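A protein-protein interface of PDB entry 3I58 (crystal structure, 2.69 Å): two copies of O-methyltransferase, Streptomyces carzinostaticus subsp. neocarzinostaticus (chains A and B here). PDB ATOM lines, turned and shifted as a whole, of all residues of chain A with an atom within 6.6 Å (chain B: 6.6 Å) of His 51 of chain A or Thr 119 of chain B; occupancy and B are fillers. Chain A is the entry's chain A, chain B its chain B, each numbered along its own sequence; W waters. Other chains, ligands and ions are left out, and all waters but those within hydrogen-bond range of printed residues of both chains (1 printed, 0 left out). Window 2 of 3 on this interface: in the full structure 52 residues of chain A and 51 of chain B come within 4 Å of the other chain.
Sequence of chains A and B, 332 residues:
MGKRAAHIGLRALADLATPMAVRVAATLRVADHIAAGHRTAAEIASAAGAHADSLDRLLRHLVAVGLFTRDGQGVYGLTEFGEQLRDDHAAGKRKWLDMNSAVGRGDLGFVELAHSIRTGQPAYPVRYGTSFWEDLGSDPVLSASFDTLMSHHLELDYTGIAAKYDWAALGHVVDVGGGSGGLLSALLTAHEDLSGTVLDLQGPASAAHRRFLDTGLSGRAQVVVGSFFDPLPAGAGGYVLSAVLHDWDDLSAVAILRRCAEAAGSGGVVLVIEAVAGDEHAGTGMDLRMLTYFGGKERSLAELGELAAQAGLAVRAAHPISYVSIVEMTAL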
ATOM      1  N   ALA A  41      -3.746  -7.609   9.241  1.00  0.00           N
ATOM      2  CA  ALA A  41      -4.675  -7.667  10.357  1.00  0.00           C
ATOM      3  C   ALA A  41      -5.693  -8.786  10.158  1.00  0.00           C
ATOM      4  O   ALA A  41      -5.931  -9.593  11.062  1.00  0.00           O
ATOM      5  CB  ALA A  41      -5.390  -6.329  10.510  1.00  0.00           C
ATOM      6  N   ALA A  45      -5.715 -11.828  12.822  1.00  0.00           N
ATOM      7  CA  ALA A  45      -6.963 -11.931  13.559  1.00  0.00           C
ATOM      8  C   ALA A  45      -7.589 -13.310  13.454  1.00  0.00           C
ATOM      9  O   ALA A  45      -7.947 -13.905  14.464  1.00  0.00           O
ATOM     10  CB  ALA A  45      -7.942 -10.878  13.065  1.00  0.00           C
ATOM     11  N   GLY A  49      -8.092 -15.583  16.395  1.00  0.00           N
ATOM     12  CA  GLY A  49      -9.451 -15.550  16.908  1.00  0.00           C
ATOM     13  C   GLY A  49      -9.881 -14.193  17.447  1.00  0.00           C
ATOM     14  O   GLY A  49     -10.703 -14.105  18.368  1.00  0.00           O
ATOM     15  N   ALA A  50      -9.332 -13.133  16.861  1.00  0.00           N
ATOM     16  CA  ALA A  50      -9.643 -11.774  17.273  1.00  0.00           C
ATOM     17  C   ALA A  50     -10.484 -11.048  16.230  1.00  0.00           C
ATOM     18  O   ALA A  50     -10.604 -11.494  15.089  1.00  0.00           O
ATOM     19  CB  ALA A  50      -8.356 -11.011  17.512  1.00  0.00           C
ATOM     20  N   HIS A  51     -11.060  -9.921  16.638  1.00  0.00           N
ATOM     21  CA  HIS A  51     -11.879  -9.081  15.766  1.00  0.00           C
ATOM     22  C   HIS A  51     -10.896  -8.316  14.886  1.00  0.00           C
ATOM     23  O   HIS A  51     -10.030  -7.607  15.393  1.00  0.00           O
ATOM     24  CB  HIS A  51     -12.711  -8.129  16.636  1.00  0.00           C
ATOM     25  CG  HIS A  51     -13.631  -7.231  15.869  1.00  0.00           C
ATOM     26  ND1 HIS A  51     -13.264  -5.970  15.447  1.00  0.00           N
ATOM     27  CD2 HIS A  51     -14.914  -7.403  15.469  1.00  0.00           C
ATOM     28  CE1 HIS A  51     -14.282  -5.404  14.823  1.00  0.00           C
ATOM     29  NE2 HIS A  51     -15.295  -6.252  14.823  1.00  0.00           N
ATOM     30  N   ALA A  52     -11.022  -8.478  13.575  1.00  0.00           N
ATOM     31  CA  ALA A  52     -10.119  -7.830  12.623  1.00  0.00           C
ATOM     32  C   ALA A  52      -9.801  -6.355  12.883  1.00  0.00           C
ATOM     33  O   ALA A  52      -8.644  -6.002  13.135  1.00  0.00           O
ATOM     34  CB  ALA A  52     -10.656  -7.993  11.212  1.00  0.00           C
ATOM     35  N   ASP A  53     -10.820  -5.499  12.813  1.00  0.00           N
ATOM     36  CA  ASP A  53     -10.638  -4.060  13.016  1.00  0.00           C
ATOM     37  C   ASP A  53     -10.027  -3.704  14.361  1.00  0.00           C
ATOM     38  O   ASP A  53      -9.154  -2.832  14.447  1.00  0.00           O
ATOM     39  CB  ASP A  53     -11.970  -3.326  12.854  1.00  0.00           C
ATOM     40  CG  ASP A  53     -12.590  -3.551  11.483  1.00  0.00           C
ATOM     41  OD1 ASP A  53     -11.842  -3.450  10.477  1.00  0.00           O
ATOM     42  OD2 ASP A  53     -13.817  -3.822  11.406  1.00  0.00           O
ATOM     43  N   SER A  54     -10.490  -4.374  15.408  1.00  0.00           N
ATOM     44  CA  SER A  54      -9.976  -4.122  16.740  1.00  0.00           C
ATOM     45  C   SER A  54      -8.499  -4.493  16.806  1.00  0.00           C
ATOM     46  O   SER A  54      -7.673  -3.703  17.256  1.00  0.00           O
ATOM     47  CB  SER A  54     -10.766  -4.926  17.773  1.00  0.00           C
ATOM     48  OG  SER A  54     -12.135  -4.562  17.774  1.00  0.00           O
ATOM     49  N   LEU A  55      -8.164  -5.695  16.346  1.00  0.00           N
ATOM     50  CA  LEU A  55      -6.773  -6.138  16.374  1.00  0.00           C
ATOM     51  C   LEU A  55      -5.903  -5.164  15.607  1.00  0.00           C
ATOM     52  O   LEU A  55      -4.833  -4.773  16.077  1.00  0.00           O
ATOM     53  CB  LEU A  55      -6.628  -7.540  15.776  1.00  0.00           C
ATOM     54  CG  LEU A  55      -5.196  -8.090  15.793  1.00  0.00           C
ATOM     55  CD1 LEU A  55      -4.642  -8.160  17.213  1.00  0.00           C
ATOM     56  CD2 LEU A  55      -5.214  -9.460  15.176  1.00  0.00           C
ATOM     57  N   ASP A  56      -6.362  -4.769  14.425  1.00  0.00           N
ATOM     58  CA  ASP A  56      -5.598  -3.825  13.632  1.00  0.00           C
ATOM     59  C   ASP A  56      -5.273  -2.598  14.490  1.00  0.00           C
ATOM     60  O   ASP A  56      -4.138  -2.107  14.492  1.00  0.00           O
ATOM     61  CB  ASP A  56      -6.373  -3.411  12.380  1.00  0.00           C
ATOM     62  CG  ASP A  56      -5.534  -2.549  11.441  1.00  0.00           C
ATOM     63  OD1 ASP A  56      -4.390  -2.951  11.118  1.00  0.00           O
ATOM     64  OD2 ASP A  56      -6.014  -1.467  11.023  1.00  0.00           O
ATOM     65  N   ALA B 114      -8.368  -7.358  26.360  1.00  0.00           N
ATOM     66  CA  ALA B 114      -8.491  -8.599  25.599  1.00  0.00           C
ATOM     67  C   ALA B 114      -9.916  -8.792  25.088  1.00  0.00           C
ATOM     68  O   ALA B 114     -10.126  -9.150  23.923  1.00  0.00           O
ATOM     69  CB  ALA B 114      -8.086  -9.777  26.453  1.00  0.00           C
ATOM     70  N   HIS B 115     -10.899  -8.542  25.950  1.00  0.00           N
ATOM     71  CA  HIS B 115     -12.284  -8.715  25.540  1.00  0.00           C
ATOM     72  C   HIS B 115     -12.613  -7.860  24.334  1.00  0.00           C
ATOM     73  O   HIS B 115     -13.338  -8.293  23.442  1.00  0.00           O
ATOM     74  CB  HIS B 115     -13.247  -8.362  26.664  1.00  0.00           C
ATOM     75  CG  HIS B 115     -14.678  -8.363  26.234  1.00  0.00           C
ATOM     76  ND1 HIS B 115     -15.351  -9.517  25.897  1.00  0.00           N
ATOM     77  CD2 HIS B 115     -15.544  -7.344  26.012  1.00  0.00           C
ATOM     78  CE1 HIS B 115     -16.568  -9.210  25.482  1.00  0.00           C
ATOM     79  NE2 HIS B 115     -16.710  -7.898  25.542  1.00  0.00           N
ATOM     80  N   SER B 116     -12.080  -6.645  24.305  1.00  0.00           N
ATOM     81  CA  SER B 116     -12.351  -5.745  23.193  1.00  0.00           C
ATOM     82  C   SER B 116     -11.635  -6.161  21.928  1.00  0.00           C
ATOM     83  O   SER B 116     -12.179  -6.048  20.830  1.00  0.00           O
ATOM     84  CB  SER B 116     -11.955  -4.309  23.550  1.00  0.00           C
ATOM     85  OG  SER B 116     -12.880  -3.739  24.453  1.00  0.00           O
ATOM     86  N   ILE B 117     -10.411  -6.643  22.075  1.00  0.00           N
ATOM     87  CA  ILE B 117      -9.652  -7.047  20.911  1.00  0.00           C
ATOM     88  C   ILE B 117     -10.238  -8.291  20.279  1.00  0.00           C
ATOM     89  O   ILE B 117     -10.183  -8.461  19.065  1.00  0.00           O
ATOM     90  CB  ILE B 117      -8.203  -7.277  21.279  1.00  0.00           C
ATOM     91  CG1 ILE B 117      -7.642  -5.991  21.885  1.00  0.00           C
ATOM     92  CG2 ILE B 117      -7.413  -7.673  20.050  1.00  0.00           C
ATOM     93  CD1 ILE B 117      -7.881  -4.765  21.006  1.00  0.00           C
ATOM     94  N   ARG B 118     -10.823  -9.151  21.101  1.00  0.00           N
ATOM     95  CA  ARG B 118     -11.425 -10.372  20.599  1.00  0.00           C
ATOM     96  C   ARG B 118     -12.796 -10.149  19.990  1.00  0.00           C
ATOM     97  O   ARG B 118     -13.098 -10.706  18.935  1.00  0.00           O
ATOM     98  CB  ARG B 118     -11.554 -11.412  21.721  1.00  0.00           C
ATOM     99  CG  ARG B 118     -10.298 -12.230  21.954  1.00  0.00           C
ATOM    100  CD  ARG B 118     -10.373 -13.060  23.227  1.00  0.00           C
ATOM    101  NE  ARG B 118      -9.128 -13.802  23.443  1.00  0.00           N
ATOM    102  CZ  ARG B 118      -8.612 -14.085  24.643  1.00  0.00           C
ATOM    103  NH1 ARG B 118      -9.227 -13.687  25.759  1.00  0.00           N
ATOM    104  NH2 ARG B 118      -7.469 -14.765  24.727  1.00  0.00           N
ATOM    105  N   THR B 119     -13.611  -9.316  20.631  1.00  0.00           N
ATOM    106  CA  THR B 119     -14.981  -9.099  20.180  1.00  0.00           C
ATOM    107  C   THR B 119     -15.364  -7.785  19.520  1.00  0.00           C
ATOM    108  O   THR B 119     -16.454  -7.686  18.955  1.00  0.00           O
ATOM    109  CB  THR B 119     -15.948  -9.273  21.343  1.00  0.00           C
ATOM    110  OG1 THR B 119     -15.857  -8.129  22.203  1.00  0.00           O
ATOM    111  CG2 THR B 119     -15.602 -10.528  22.139  1.00  0.00           C
ATOM    112  N   GLY B 120     -14.498  -6.778  19.598  1.00  0.00           N
ATOM    113  CA  GLY B 120     -14.831  -5.488  19.020  1.00  0.00           C
ATOM    114  C   GLY B 120     -15.769  -4.723  19.949  1.00  0.00           C
ATOM    115  O   GLY B 120     -16.110  -3.569  19.694  1.00  0.00           O
ATOM    116  N   GLN B 121     -16.195  -5.371  21.032  1.00  0.00           N
ATOM    117  CA  GLN B 121     -17.086  -4.749  22.008  1.00  0.00           C
ATOM    118  C   GLN B 121     -16.304  -3.987  23.087  1.00  0.00           C
ATOM    119  O   GLN B 121     -15.113  -4.227  23.295  1.00  0.00           O
ATOM    120  CB  GLN B 121     -17.967  -5.815  22.658  1.00  0.00           C
ATOM    121  CG  GLN B 121     -19.089  -6.320  21.764  1.00  0.00           C
ATOM    122  CD  GLN B 121     -20.061  -5.208  21.340  1.00  0.00           C
ATOM    123  OE1 GLN B 121     -19.737  -4.352  20.505  1.00  0.00           O
ATOM    124  NE2 GLN B 121     -21.259  -5.215  21.928  1.00  0.00           N
ATOM    125  N   PRO B 122     -16.966  -3.047  23.783  1.00  0.00           N
ATOM    126  CA  PRO B 122     -16.309  -2.261  24.836  1.00  0.00           C
ATOM    127  C   PRO B 122     -15.942  -3.087  26.063  1.00  0.00           C
ATOM    128  O   PRO B 122     -16.639  -4.033  26.420  1.00  0.00           O
ATOM    129  CB  PRO B 122     -17.339  -1.180  25.147  1.00  0.00           C
ATOM    130  CG  PRO B 122     -18.628  -1.874  24.893  1.00  0.00           C
ATOM    131  CD  PRO B 122     -18.359  -2.601  23.599  1.00  0.00           C
HETATM  132  O   HOH W   1     -11.021 -15.537  21.115  1.00  0.00           O
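No position is printed for both chains. Of the 10 pairs that touch across the chains among the printed residues, none has its exchanged pair printed and touching as well.
N of His 51 of chain A lies within hydrogen-bond range of O of Ile 117 of chain B (3.0 Å). N of His 51 of chain A is in hydrogen-bond range of O of Arg 118 of chain B, 3.2 Å away. OG of Ser 54 of chain A sits at hydrogen-bond distance from O of Ser 116 of chain B, 3.4 Å away.
Printed residues of chain B within 4 Å of Ser 54 of chain A: Ser 116 (3.4 Å), Ile 117 (3.8 Å) and Gly 120 (3.1 Å). Of the printed residues of chain B, Leu 55 of chain A touches Ile 117 (3.996 Å). Thr 119 of chain B touches just one residue of chain A: His 51 (3.8 Å). Printed residues of chain A within 4 Å of Gly 120 of chain B: His 51 and Ser 54. The nearest residue of chain A that does not touch Thr 119 of chain B is Ser 54 of chain A (4.9 Å). The nearest printed residue of chain A that does not touch Gly 120 of chain B is Ala 50 of chain A (6.8 Å).
Ile 117 of chain B touches Ala 50 of chain A. O of Arg 118 of chain B touches C of Ala 50 of chain A, 3.8 Å away. CD2 of His 51 of chain A touches O of Thr 119 of chain B, at 3.8 Å. Gly 120 of chain B touches His 51 of chain A (N to CB, 3.7 Å). Ser 54 of chain A touches Ile 117 of chain B (CB to O, 3.8 Å). Ser 54 of chain A touches Gly 120 of chain B. Leu 55 of chain A touches Ile 117 of chain B.
Water W1 bridges the backbone carbonyl oxygen of Gly 49 of chain A and the guanidinium group of Arg 118 of chain B.
O of Ala 45 of chain A is in hydrogen-bond range of N of Ala 50 of chain A (2.9 Å). A ring nitrogen (ND1) of His 51 of chain A sits at hydrogen-bond distance from the side-chain hydroxyl (OG) of Ser 54 of chain A, at 2.9 Å. OG1 of Thr 119 of chain B is in hydrogen-bond range of O of His 115 of chain B (2.8 Å). The side-chain hydroxyl (OG) of Ser 116 of chain B sits at hydrogen-bond distance from the backbone carbonyl oxygen (O) of Gln 121 of chain B (2.6 Å). OG1 of Thr 119 of chain B lies close to N of Gln 121 of chain B (3.0 Å).
Hydrophobic or aromatic side chains of chain A that line the printed part of chain B: Ala 50, His 51 and Leu 55. Of the 9 printed residues of chain B, 5 touch a printed residue of chain A. Printed residues of chain B that touch a printed residue of chain A: Ser 116, Ile 117, Arg 118, Thr 119 and Gly 120. Hydrophobic or aromatic side chains of chain B that line the printed part of chain A: Ile 117. Along chain B the printed residues that touch a printed residue of chain A span positions 116 to 120. Among the printed residues, 10 pairs touch across the chains.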
